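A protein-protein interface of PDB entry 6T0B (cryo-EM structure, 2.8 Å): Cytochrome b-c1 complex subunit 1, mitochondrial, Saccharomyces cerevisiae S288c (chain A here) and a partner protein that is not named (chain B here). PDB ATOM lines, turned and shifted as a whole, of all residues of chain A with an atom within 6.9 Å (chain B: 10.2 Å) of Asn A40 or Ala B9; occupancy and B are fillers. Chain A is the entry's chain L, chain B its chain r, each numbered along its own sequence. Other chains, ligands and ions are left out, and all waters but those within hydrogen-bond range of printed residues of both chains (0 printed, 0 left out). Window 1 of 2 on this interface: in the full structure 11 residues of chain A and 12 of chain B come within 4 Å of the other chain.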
ATOM      1  N   ASN A  35     -19.630 -17.159  19.694  1.00  0.00           N
ATOM      2  CA  ASN A  35     -20.159 -16.050  20.467  1.00  0.00           C
ATOM      3  C   ASN A  35     -21.150 -15.258  19.644  1.00  0.00           C
ATOM      4  O   ASN A  35     -21.215 -14.036  19.726  1.00  0.00           O
ATOM      5  CB  ASN A  35     -19.041 -15.147  20.961  1.00  0.00           C
ATOM      6  CG  ASN A  35     -18.081 -15.864  21.847  1.00  0.00           C
ATOM      7  OD1 ASN A  35     -17.269 -16.647  21.385  1.00  0.00           O
ATOM      8  ND2 ASN A  35     -18.172 -15.616  23.137  1.00  0.00           N
ATOM      9  N   GLU A  36     -21.923 -15.942  18.819  1.00  0.00           N
ATOM     10  CA  GLU A  36     -22.902 -15.291  17.974  1.00  0.00           C
ATOM     11  C   GLU A  36     -24.260 -15.938  18.181  1.00  0.00           C
ATOM     12  O   GLU A  36     -24.382 -16.999  18.786  1.00  0.00           O
ATOM     13  CB  GLU A  36     -22.496 -15.360  16.505  1.00  0.00           C
ATOM     14  CG  GLU A  36     -21.175 -14.713  16.227  1.00  0.00           C
ATOM     15  CD  GLU A  36     -20.656 -15.014  14.854  1.00  0.00           C
ATOM     16  OE1 GLU A  36     -21.432 -15.534  14.035  1.00  0.00           O
ATOM     17  OE2 GLU A  36     -19.473 -14.728  14.590  1.00  0.00           O
ATOM     18  N   ASN A  37     -25.284 -15.271  17.695  1.00  0.00           N
ATOM     19  CA  ASN A  37     -26.638 -15.792  17.678  1.00  0.00           C
ATOM     20  C   ASN A  37     -26.794 -16.603  16.405  1.00  0.00           C
ATOM     21  O   ASN A  37     -25.877 -16.624  15.583  1.00  0.00           O
ATOM     22  CB  ASN A  37     -27.648 -14.647  17.715  1.00  0.00           C
ATOM     23  CG  ASN A  37     -27.308 -13.611  18.739  1.00  0.00           C
ATOM     24  OD1 ASN A  37     -26.906 -12.503  18.408  1.00  0.00           O
ATOM     25  ND2 ASN A  37     -27.478 -13.962  20.002  1.00  0.00           N
ATOM     26  N   PRO A  38     -27.926 -17.274  16.184  1.00  0.00           N
ATOM     27  CA  PRO A  38     -28.245 -17.733  14.830  1.00  0.00           C
ATOM     28  C   PRO A  38     -28.693 -16.633  13.895  1.00  0.00           C
ATOM     29  O   PRO A  38     -29.011 -16.923  12.741  1.00  0.00           O
ATOM     30  CB  PRO A  38     -29.383 -18.722  15.069  1.00  0.00           C
ATOM     31  CG  PRO A  38     -29.168 -19.195  16.416  1.00  0.00           C
ATOM     32  CD  PRO A  38     -28.707 -18.016  17.181  1.00  0.00           C
ATOM     33  N   TYR A  39     -28.744 -15.386  14.347  1.00  0.00           N
ATOM     34  CA  TYR A  39     -29.285 -14.291  13.567  1.00  0.00           C
ATOM     35  C   TYR A  39     -28.237 -13.298  13.116  1.00  0.00           C
ATOM     36  O   TYR A  39     -28.407 -12.689  12.065  1.00  0.00           O
ATOM     37  CB  TYR A  39     -30.362 -13.565  14.371  1.00  0.00           C
ATOM     38  CG  TYR A  39     -31.513 -14.470  14.717  1.00  0.00           C
ATOM     39  CD1 TYR A  39     -32.547 -14.669  13.822  1.00  0.00           C
ATOM     40  CD2 TYR A  39     -31.555 -15.147  15.924  1.00  0.00           C
ATOM     41  CE1 TYR A  39     -33.599 -15.497  14.124  1.00  0.00           C
ATOM     42  CE2 TYR A  39     -32.600 -15.981  16.232  1.00  0.00           C
ATOM     43  CZ  TYR A  39     -33.616 -16.152  15.328  1.00  0.00           C
ATOM     44  OH  TYR A  39     -34.663 -16.982  15.631  1.00  0.00           O
ATOM     45  N   ASN A  40     -27.160 -13.121  13.874  1.00  0.00           N
ATOM     46  CA  ASN A  40     -25.992 -12.405  13.391  1.00  0.00           C
ATOM     47  C   ASN A  40     -24.866 -13.357  13.020  1.00  0.00           C
ATOM     48  O   ASN A  40     -23.691 -13.015  13.136  1.00  0.00           O
ATOM     49  CB  ASN A  40     -25.531 -11.371  14.416  1.00  0.00           C
ATOM     50  CG  ASN A  40     -24.926 -11.985  15.642  1.00  0.00           C
ATOM     51  OD1 ASN A  40     -25.318 -13.057  16.063  1.00  0.00           O
ATOM     52  ND2 ASN A  40     -23.940 -11.318  16.204  1.00  0.00           N
ATOM     53  N   ASN A  41     -25.206 -14.557  12.569  1.00  0.00           N
ATOM     54  CA  ASN A  41     -24.190 -15.518  12.171  1.00  0.00           C
ATOM     55  C   ASN A  41     -23.514 -15.048  10.900  1.00  0.00           C
ATOM     56  O   ASN A  41     -24.180 -14.768   9.902  1.00  0.00           O
ATOM     57  CB  ASN A  41     -24.806 -16.884  11.961  1.00  0.00           C
ATOM     58  CG  ASN A  41     -23.822 -17.986  12.188  1.00  0.00           C
ATOM     59  OD1 ASN A  41     -22.683 -17.745  12.553  1.00  0.00           O
ATOM     60  ND2 ASN A  41     -24.257 -19.208  11.990  1.00  0.00           N
ATOM     61  N   GLY A  42     -22.198 -14.911  10.961  1.00  0.00           N
ATOM     62  CA  GLY A  42     -21.432 -14.359   9.872  1.00  0.00           C
ATOM     63  C   GLY A  42     -20.892 -12.978  10.114  1.00  0.00           C
ATOM     64  O   GLY A  42     -20.411 -12.351   9.169  1.00  0.00           O
ATOM     65  N   VAL A  43     -20.962 -12.480  11.345  1.00  0.00           N
ATOM     66  CA  VAL A  43     -20.395 -11.179  11.667  1.00  0.00           C
ATOM     67  C   VAL A  43     -18.877 -11.243  11.667  1.00  0.00           C
ATOM     68  O   VAL A  43     -18.210 -10.361  11.119  1.00  0.00           O
ATOM     69  CB  VAL A  43     -20.957 -10.688  13.009  1.00  0.00           C
ATOM     70  CG1 VAL A  43     -20.149  -9.584  13.525  1.00  0.00           C
ATOM     71  CG2 VAL A  43     -22.335 -10.155  12.814  1.00  0.00           C
ATOM     72  N   SER A  44     -18.309 -12.297  12.247  1.00  0.00           N
ATOM     73  CA  SER A  44     -16.860 -12.436  12.269  1.00  0.00           C
ATOM     74  C   SER A  44     -16.282 -12.641  10.875  1.00  0.00           C
ATOM     75  O   SER A  44     -15.159 -12.213  10.609  1.00  0.00           O
ATOM     76  CB  SER A  44     -16.466 -13.587  13.178  1.00  0.00           C
ATOM     77  OG  SER A  44     -16.855 -13.329  14.506  1.00  0.00           O
ATOM     78  N   LEU A 150     -22.453 -23.207  15.425  1.00  0.00           N
ATOM     79  CA  LEU A 150     -22.624 -22.218  14.384  1.00  0.00           C
ATOM     80  C   LEU A 150     -21.491 -22.297  13.383  1.00  0.00           C
ATOM     81  O   LEU A 150     -20.331 -22.436  13.783  1.00  0.00           O
ATOM     82  CB  LEU A 150     -22.684 -20.814  14.977  1.00  0.00           C
ATOM     83  CG  LEU A 150     -23.876 -20.681  15.906  1.00  0.00           C
ATOM     84  CD1 LEU A 150     -23.626 -19.632  16.917  1.00  0.00           C
ATOM     85  CD2 LEU A 150     -25.107 -20.373  15.116  1.00  0.00           C
ATOM     86  N   GLY A 154     -20.696 -18.392   8.571  1.00  0.00           N
ATOM     87  CA  GLY A 154     -22.015 -17.819   8.615  1.00  0.00           C
ATOM     88  C   GLY A 154     -22.978 -18.581   7.746  1.00  0.00           C
ATOM     89  O   GLY A 154     -22.792 -19.769   7.501  1.00  0.00           O
ATOM     90  N   SER A 158     -28.523 -15.795   6.960  1.00  0.00           N
ATOM     91  CA  SER A 158     -28.126 -14.916   8.049  1.00  0.00           C
ATOM     92  C   SER A 158     -27.359 -13.705   7.548  1.00  0.00           C
ATOM     93  O   SER A 158     -27.565 -12.593   8.039  1.00  0.00           O
ATOM     94  CB  SER A 158     -27.272 -15.689   9.038  1.00  0.00           C
ATOM     95  OG  SER A 158     -26.697 -14.824   9.984  1.00  0.00           O
ATOM     96  N   LEU A 159     -26.461 -13.903   6.585  1.00  0.00           N
ATOM     97  CA  LEU A 159     -25.544 -12.853   6.164  1.00  0.00           C
ATOM     98  C   LEU A 159     -26.219 -11.735   5.398  1.00  0.00           C
ATOM     99  O   LEU A 159     -25.654 -10.648   5.315  1.00  0.00           O
ATOM    100  CB  LEU A 159     -24.441 -13.425   5.291  1.00  0.00           C
ATOM    101  CG  LEU A 159     -23.246 -13.990   6.029  1.00  0.00           C
ATOM    102  CD1 LEU A 159     -22.403 -14.789   5.086  1.00  0.00           C
ATOM    103  CD2 LEU A 159     -22.458 -12.860   6.596  1.00  0.00           C
ATOM    104  N   ASN A 161     -28.976 -10.213   6.169  1.00  0.00           N
ATOM    105  CA  ASN A 161     -29.667  -9.288   7.045  1.00  0.00           C
ATOM    106  C   ASN A 161     -28.707  -8.416   7.827  1.00  0.00           C
ATOM    107  O   ASN A 161     -29.151  -7.573   8.605  1.00  0.00           O
ATOM    108  CB  ASN A 161     -30.572 -10.043   8.015  1.00  0.00           C
ATOM    109  CG  ASN A 161     -31.743 -10.675   7.329  1.00  0.00           C
ATOM    110  OD1 ASN A 161     -32.292 -11.662   7.804  1.00  0.00           O
ATOM    111  ND2 ASN A 161     -32.139 -10.111   6.200  1.00  0.00           N
ATOM    112  N   LEU A 162     -27.410  -8.599   7.641  1.00  0.00           N
ATOM    113  CA  LEU A 162     -26.423  -7.871   8.415  1.00  0.00           C
ATOM    114  C   LEU A 162     -26.244  -6.469   7.870  1.00  0.00           C
ATOM    115  O   LEU A 162     -26.312  -6.244   6.661  1.00  0.00           O
ATOM    116  CB  LEU A 162     -25.091  -8.605   8.393  1.00  0.00           C
ATOM    117  CG  LEU A 162     -24.723  -9.423   9.617  1.00  0.00           C
ATOM    118  CD1 LEU A 162     -25.822 -10.364   9.998  1.00  0.00           C
ATOM    119  CD2 LEU A 162     -23.502 -10.207   9.290  1.00  0.00           C
ATOM    120  N   VAL A 163     -26.032  -5.521   8.774  1.00  0.00           N
ATOM    121  CA  VAL A 163     -25.750  -4.137   8.451  1.00  0.00           C
ATOM    122  C   VAL A 163     -24.503  -3.728   9.224  1.00  0.00           C
ATOM    123  O   VAL A 163     -23.901  -4.539   9.920  1.00  0.00           O
ATOM    124  CB  VAL A 163     -26.938  -3.213   8.771  1.00  0.00           C
ATOM    125  CG1 VAL A 163     -28.106  -3.514   7.864  1.00  0.00           C
ATOM    126  CG2 VAL A 163     -27.346  -3.389  10.195  1.00  0.00           C
ATOM    127  N   ASP A 166     -24.627  -4.031  13.153  1.00  0.00           N
ATOM    128  CA  ASP A 166     -24.313  -5.319  13.756  1.00  0.00           C
ATOM    129  C   ASP A 166     -22.818  -5.510  13.902  1.00  0.00           C
ATOM    130  O   ASP A 166     -22.352  -6.057  14.910  1.00  0.00           O
ATOM    131  CB  ASP A 166     -24.902  -6.436  12.916  1.00  0.00           C
ATOM    132  CG  ASP A 166     -26.392  -6.450  12.957  1.00  0.00           C
ATOM    133  OD1 ASP A 166     -26.951  -6.643  14.050  1.00  0.00           O
ATOM    134  OD2 ASP A 166     -27.020  -6.248  11.906  1.00  0.00           O
ATOM    135  N   PHE A 170     -21.032  -5.888  17.564  1.00  0.00           N
ATOM    136  CA  PHE A 170     -20.120  -6.973  17.890  1.00  0.00           C
ATOM    137  C   PHE A 170     -18.747  -6.443  18.252  1.00  0.00           C
ATOM    138  O   PHE A 170     -18.072  -7.003  19.121  1.00  0.00           O
ATOM    139  CB  PHE A 170     -20.026  -7.918  16.705  1.00  0.00           C
ATOM    140  CG  PHE A 170     -19.241  -9.172  16.976  1.00  0.00           C
ATOM    141  CD1 PHE A 170     -19.864 -10.291  17.475  1.00  0.00           C
ATOM    142  CD2 PHE A 170     -17.892  -9.246  16.693  1.00  0.00           C
ATOM    143  CE1 PHE A 170     -19.156 -11.439  17.720  1.00  0.00           C
ATOM    144  CE2 PHE A 170     -17.186 -10.387  16.949  1.00  0.00           C
ATOM    145  CZ  PHE A 170     -17.819 -11.482  17.459  1.00  0.00           C
ATOM    146  N   ALA B   5     -33.547   3.418  14.512  1.00  0.00           N
ATOM    147  CA  ALA B   5     -34.040   2.079  14.783  1.00  0.00           C
ATOM    148  C   ALA B   5     -32.904   1.074  14.879  1.00  0.00           C
ATOM    149  O   ALA B   5     -31.790   1.302  14.410  1.00  0.00           O
ATOM    150  CB  ALA B   5     -35.013   1.646  13.692  1.00  0.00           C
ATOM    151  N   LEU B   6     -33.201  -0.052  15.509  1.00  0.00           N
ATOM    152  CA  LEU B   6     -32.187  -1.062  15.742  1.00  0.00           C
ATOM    153  C   LEU B   6     -31.980  -1.903  14.486  1.00  0.00           C
ATOM    154  O   LEU B   6     -32.669  -1.740  13.474  1.00  0.00           O
ATOM    155  CB  LEU B   6     -32.564  -1.927  16.941  1.00  0.00           C
ATOM    156  CG  LEU B   6     -32.061  -1.465  18.313  1.00  0.00           C
ATOM    157  CD1 LEU B   6     -30.557  -1.313  18.247  1.00  0.00           C
ATOM    158  CD2 LEU B   6     -32.735  -0.182  18.810  1.00  0.00           C
ATOM    159  N   SER B   7     -30.982  -2.784  14.542  1.00  0.00           N
ATOM    160  CA  SER B   7     -30.780  -3.761  13.484  1.00  0.00           C
ATOM    161  C   SER B   7     -31.959  -4.708  13.413  1.00  0.00           C
ATOM    162  O   SER B   7     -32.632  -4.972  14.409  1.00  0.00           O
ATOM    163  CB  SER B   7     -29.515  -4.573  13.730  1.00  0.00           C
ATOM    164  OG  SER B   7     -29.331  -5.520  12.698  1.00  0.00           O
ATOM    165  N   LYS B   8     -32.213  -5.217  12.215  1.00  0.00           N
ATOM    166  CA  LYS B   8     -33.147  -6.323  12.098  1.00  0.00           C
ATOM    167  C   LYS B   8     -32.579  -7.561  12.766  1.00  0.00           C
ATOM    168  O   LYS B   8     -33.198  -8.131  13.666  1.00  0.00           O
ATOM    169  CB  LYS B   8     -33.462  -6.599  10.634  1.00  0.00           C
ATOM    170  CG  LYS B   8     -34.839  -7.171  10.427  1.00  0.00           C
ATOM    171  CD  LYS B   8     -35.168  -7.316   8.964  1.00  0.00           C
ATOM    172  CE  LYS B   8     -34.283  -8.351   8.320  1.00  0.00           C
ATOM    173  NZ  LYS B   8     -34.272  -9.597   9.116  1.00  0.00           N
ATOM    174  N   ALA B   9     -31.359  -7.939  12.405  1.00  0.00           N
ATOM    175  CA  ALA B   9     -30.827  -9.213  12.858  1.00  0.00           C
ATOM    176  C   ALA B   9     -30.166  -9.136  14.227  1.00  0.00           C
ATOM    177  O   ALA B   9     -29.064  -9.653  14.424  1.00  0.00           O
ATOM    178  CB  ALA B   9     -29.830  -9.738  11.830  1.00  0.00           C
ATOM    179  N   THR B  10     -30.836  -8.492  15.170  1.00  0.00           N
ATOM    180  CA  THR B  10     -30.641  -8.738  16.586  1.00  0.00           C
ATOM    181  C   THR B  10     -31.955  -8.615  17.330  1.00  0.00           C
ATOM    182  O   THR B  10     -31.959  -8.703  18.559  1.00  0.00           O
ATOM    183  CB  THR B  10     -29.601  -7.786  17.198  1.00  0.00           C
ATOM    184  OG1 THR B  10     -29.530  -8.007  18.608  1.00  0.00           O
ATOM    185  CG2 THR B  10     -29.966  -6.358  16.946  1.00  0.00           C
ATOM    186  N   LEU B  11     -33.065  -8.392  16.621  1.00  0.00           N
ATOM    187  CA  LEU B  11     -34.386  -8.362  17.225  1.00  0.00           C
ATOM    188  C   LEU B  11     -35.414  -9.213  16.514  1.00  0.00           C
ATOM    189  O   LEU B  11     -36.565  -9.221  16.959  1.00  0.00           O
ATOM    190  CB  LEU B  11     -34.967  -6.944  17.280  1.00  0.00           C
ATOM    191  CG  LEU B  11     -34.597  -6.028  18.431  1.00  0.00           C
ATOM    192  CD1 LEU B  11     -34.814  -6.733  19.755  1.00  0.00           C
ATOM    193  CD2 LEU B  11     -33.222  -5.510  18.263  1.00  0.00           C
ATOM    194  N   THR B  12     -35.078  -9.851  15.396  1.00  0.00           N
ATOM    195  CA  THR B  12     -35.996 -10.808  14.801  1.00  0.00           C
ATOM    196  C   THR B  12     -36.241 -11.936  15.782  1.00  0.00           C
ATOM    197  O   THR B  12     -35.290 -12.569  16.247  1.00  0.00           O
ATOM    198  CB  THR B  12     -35.434 -11.376  13.504  1.00  0.00           C
ATOM    199  OG1 THR B  12     -34.170 -11.979  13.772  1.00  0.00           O
ATOM    200  CG2 THR B  12     -35.270 -10.309  12.455  1.00  0.00           C
ATOM    201  N   ASP B  13     -37.517 -12.138  16.122  1.00  0.00           N
ATOM    202  CA  ASP B  13     -37.979 -13.181  17.034  1.00  0.00           C
ATOM    203  C   ASP B  13     -37.304 -13.039  18.400  1.00  0.00           C
ATOM    204  O   ASP B  13     -36.553 -13.899  18.845  1.00  0.00           O
ATOM    205  CB  ASP B  13     -37.758 -14.567  16.416  1.00  0.00           C
ATOM    206  CG  ASP B  13     -38.541 -15.663  17.102  1.00  0.00           C
ATOM    207  OD1 ASP B  13     -39.062 -15.452  18.210  1.00  0.00           O
ATOM    208  OD2 ASP B  13     -38.644 -16.758  16.515  1.00  0.00           O
ATOM    209  N   LEU B  14     -37.561 -11.918  19.035  1.00  0.00           N
ATOM    210  CA  LEU B  14     -37.086 -11.720  20.397  1.00  0.00           C
ATOM    211  C   LEU B  14     -37.820 -12.558  21.449  1.00  0.00           C
ATOM    212  O   LEU B  14     -37.142 -13.107  22.329  1.00  0.00           O
ATOM    213  CB  LEU B  14     -37.147 -10.238  20.772  1.00  0.00           C
ATOM    214  CG  LEU B  14     -36.291  -9.922  21.989  1.00  0.00           C
ATOM    215  CD1 LEU B  14     -34.821 -10.023  21.633  1.00  0.00           C
ATOM    216  CD2 LEU B  14     -36.628  -8.559  22.519  1.00  0.00           C
ATOM    217  N   ARG B  17     -35.964 -16.127  21.976  1.00  0.00           N
ATOM    218  CA  ARG B  17     -34.569 -16.210  22.374  1.00  0.00           C
ATOM    219  C   ARG B  17     -34.210 -15.189  23.438  1.00  0.00           C
ATOM    220  O   ARG B  17     -33.027 -14.975  23.706  1.00  0.00           O
ATOM    221  CB  ARG B  17     -33.666 -16.029  21.166  1.00  0.00           C
ATOM    222  CG  ARG B  17     -33.877 -14.726  20.469  1.00  0.00           C
ATOM    223  CD  ARG B  17     -32.778 -14.494  19.481  1.00  0.00           C
ATOM    224  NE  ARG B  17     -33.159 -13.533  18.467  1.00  0.00           N
ATOM    225  CZ  ARG B  17     -32.368 -12.557  18.051  1.00  0.00           C
ATOM    226  NH1 ARG B  17     -32.786 -11.727  17.115  1.00  0.00           N
ATOM    227  NH2 ARG B  17     -31.162 -12.413  18.575  1.00  0.00           N
ATOM    228  N   MET B  21     -30.197 -15.593  26.612  1.00  0.00           N
ATOM    229  CA  MET B  21     -29.641 -14.280  26.336  1.00  0.00           C
ATOM    230  C   MET B  21     -28.524 -14.042  27.338  1.00  0.00           C
ATOM    231  O   MET B  21     -28.786 -14.014  28.554  1.00  0.00           O
ATOM    232  CB  MET B  21     -30.700 -13.188  26.433  1.00  0.00           C
ATOM    233  CG  MET B  21     -30.302 -11.909  25.774  1.00  0.00           C
ATOM    234  SD  MET B  21     -30.170 -12.077  23.990  1.00  0.00           S
ATOM    235  CE  MET B  21     -31.825 -11.669  23.472  1.00  0.00           C
ATOM    236  N   PRO B  22     -27.298 -13.814  26.885  1.00  0.00           N
ATOM    237  CA  PRO B  22     -26.157 -13.594  27.786  1.00  0.00           C
ATOM    238  C   PRO B  22     -26.195 -12.461  28.811  1.00  0.00           C
ATOM    239  O   PRO B  22     -25.160 -12.177  29.421  1.00  0.00           O
ATOM    240  CB  PRO B  22     -25.025 -13.362  26.784  1.00  0.00           C
ATOM    241  CG  PRO B  22     -25.378 -14.279  25.634  1.00  0.00           C
ATOM    242  CD  PRO B  22     -26.864 -14.560  25.693  1.00  0.00           C
ATOM    243  N   GLU B  25     -26.642  -7.899  27.181  1.00  0.00           N
ATOM    244  CA  GLU B  25     -27.362  -7.306  26.069  1.00  0.00           C
ATOM    245  C   GLU B  25     -28.858  -7.234  26.292  1.00  0.00           C
ATOM    246  O   GLU B  25     -29.543  -6.599  25.490  1.00  0.00           O
ATOM    247  CB  GLU B  25     -27.079  -8.095  24.799  1.00  0.00           C
ATOM    248  CG  GLU B  25     -27.823  -9.385  24.731  1.00  0.00           C
ATOM    249  CD  GLU B  25     -27.135 -10.513  25.468  1.00  0.00           C
ATOM    250  OE1 GLU B  25     -26.835 -10.399  26.676  1.00  0.00           O
ATOM    251  OE2 GLU B  25     -26.895 -11.526  24.806  1.00  0.00           O
ATOM    252  N   ILE B  29     -30.499  -3.873  25.178  1.00  0.00           N
ATOM    253  CA  ILE B  29     -31.665  -3.887  24.310  1.00  0.00           C
ATOM    254  C   ILE B  29     -32.912  -3.336  25.007  1.00  0.00           C
ATOM    255  O   ILE B  29     -33.876  -2.963  24.322  1.00  0.00           O
ATOM    256  CB  ILE B  29     -31.917  -5.300  23.740  1.00  0.00           C
ATOM    257  CG1 ILE B  29     -32.769  -5.237  22.478  1.00  0.00           C
ATOM    258  CG2 ILE B  29     -32.641  -6.147  24.730  1.00  0.00           C
ATOM    259  CD1 ILE B  29     -32.264  -4.234  21.499  1.00  0.00           C
ATOM    260  N   ASN B  45     -41.281   0.895  13.688  1.00  0.00           N
ATOM    261  CA  ASN B  45     -41.628  -0.294  12.932  1.00  0.00           C
ATOM    262  C   ASN B  45     -42.190  -1.348  13.867  1.00  0.00           C
ATOM    263  O   ASN B  45     -41.827  -1.423  15.040  1.00  0.00           O
ATOM    264  CB  ASN B  45     -40.409  -0.845  12.213  1.00  0.00           C
ATOM    265  CG  ASN B  45     -39.248  -1.034  13.139  1.00  0.00           C
ATOM    266  OD1 ASN B  45     -39.179  -0.403  14.189  1.00  0.00           O
ATOM    267  ND2 ASN B  45     -38.324  -1.908  12.765  1.00  0.00           N
ATOM    268  N   GLU B  47     -41.714  -4.367  14.302  1.00  0.00           N
ATOM    269  CA  GLU B  47     -40.871  -5.398  14.885  1.00  0.00           C
ATOM    270  C   GLU B  47     -40.495  -5.050  16.320  1.00  0.00           C
ATOM    271  O   GLU B  47     -40.416  -5.936  17.178  1.00  0.00           O
ATOM    272  CB  GLU B  47     -39.629  -5.597  14.026  1.00  0.00           C
ATOM    273  CG  GLU B  47     -38.709  -6.691  14.514  1.00  0.00           C
ATOM    274  CD  GLU B  47     -37.436  -6.770  13.714  1.00  0.00           C
ATOM    275  OE1 GLU B  47     -37.480  -6.493  12.496  1.00  0.00           O
ATOM    276  OE2 GLU B  47     -36.387  -7.097  14.303  1.00  0.00           O
ATOM    277  N   GLU B  48     -40.277  -3.765  16.611  1.00  0.00           N
ATOM    278  CA  GLU B  48     -39.902  -3.401  17.972  1.00  0.00           C
ATOM    279  C   GLU B  48     -41.098  -3.288  18.895  1.00  0.00           C
ATOM    280  O   GLU B  48     -40.950  -3.483  20.102  1.00  0.00           O
ATOM    281  CB  GLU B  48     -39.143  -2.079  18.013  1.00  0.00           C
ATOM    282  CG  GLU B  48     -37.818  -2.071  17.292  1.00  0.00           C
ATOM    283  CD  GLU B  48     -36.789  -3.069  17.826  1.00  0.00           C
ATOM    284  OE1 GLU B  48     -36.820  -3.453  19.021  1.00  0.00           O
ATOM    285  OE2 GLU B  48     -35.915  -3.452  17.022  1.00  0.00           O
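The side-chain carboxylate (OD2) of Asp A166 lies within hydrogen-bond range of the side-chain hydroxyl (OG) of Ser B7 (2.5 Å). The side-chain amide oxygen (OD1) of Asn A161 sits at hydrogen-bond distance from the side-chain amino group (NZ) of Lys B8 (3.1 Å).
O of Thr B10 sits close to NH1 of Arg B17 (3.5 Å). The backbone carbonyl oxygen (O) of Thr B12 sits at hydrogen-bond distance from the guanidinium group (NH1) of Arg B17 (2.8 Å). The backbone NH (N) of Asn A37 sits at hydrogen-bond distance from the side-chain amide oxygen (OD1) of Asn A40. OG of Ser A158 lies within hydrogen-bond range of O of Tyr A39, at 3.4 Å. N of Thr B12 lies within hydrogen-bond range of OE2 of Glu B47. The side-chain hydroxyl of Ser B7 sits at hydrogen-bond distance from the backbone NH of Ala B9 (3.2 Å).
Among the printed residues, merely in contact across the chains: Tyr A39 with Ala B9 (3.3 Å), Tyr A39 with Thr B12 (3.1 Å), Tyr A39 with Arg B17 (3.4 Å), Asn A40 with Ala B9 (3.9 Å), Asn A161 with Ala B9 (3.9 Å), Val A163 with Ser B7 (3.8 Å) and Asp A166 with Ala B9 (3.7 Å).
Of chain B, only Ala B9 comes within 4 Å of Asn A40. Of chain A, only Tyr A39, Asn A40, Asn A161 and Asp A166 come within 4 Å of Ala B9. No residue of chain B comes within 4 Å of Glu A36. No residue of chain B comes within 4 Å of Asn A37. Asn A41 touches none of the printed residues of chain B. No residue of chain B comes within 4 Å of Gly A42. Asn A161 touches two residues of chain B. Printed residues of chain B within 4 Å of Asp A166: Ser B7 (2.5 Å) and Ala B9 (3.7 Å). Of the printed residues of chain A, Lys B8 touches Asn A161 (3.1 Å). Of the printed residues of chain A, Ser B7 touches Val A163 (3.8 Å) and Asp A166 (2.5 Å). Of the printed residues of chain A, Thr B12 touches Tyr A39. Of the printed residues of chain A, Arg B17 touches Tyr A39 (3.4 Å). Leu A150 touches none of the printed residues of chain B. The nearest printed residue of chain A that does not touch Ser B7 is Asn A161 (4.6 Å).
Of the 19 printed residues of chain A, 5 touch a printed residue of chain B. Printed residues of chain A that touch a printed residue of chain B: Tyr A39, Asn A40, Asn A161, Val A163 and Asp A166. Hydrophobic or aromatic side chains of chain A that line the printed part of chain B: Tyr A39 and Val A163. Of the 18 printed residues of chain B, 5 touch a printed residue of chain A. Hydrophobic or aromatic side chains of chain B within 4 Å of the printed part of chain A: Ala B9. Among the printed residues, no Asp or Glu carboxylate lies within 4 Å of a Lys or Arg side-chain nitrogen of the other chain.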
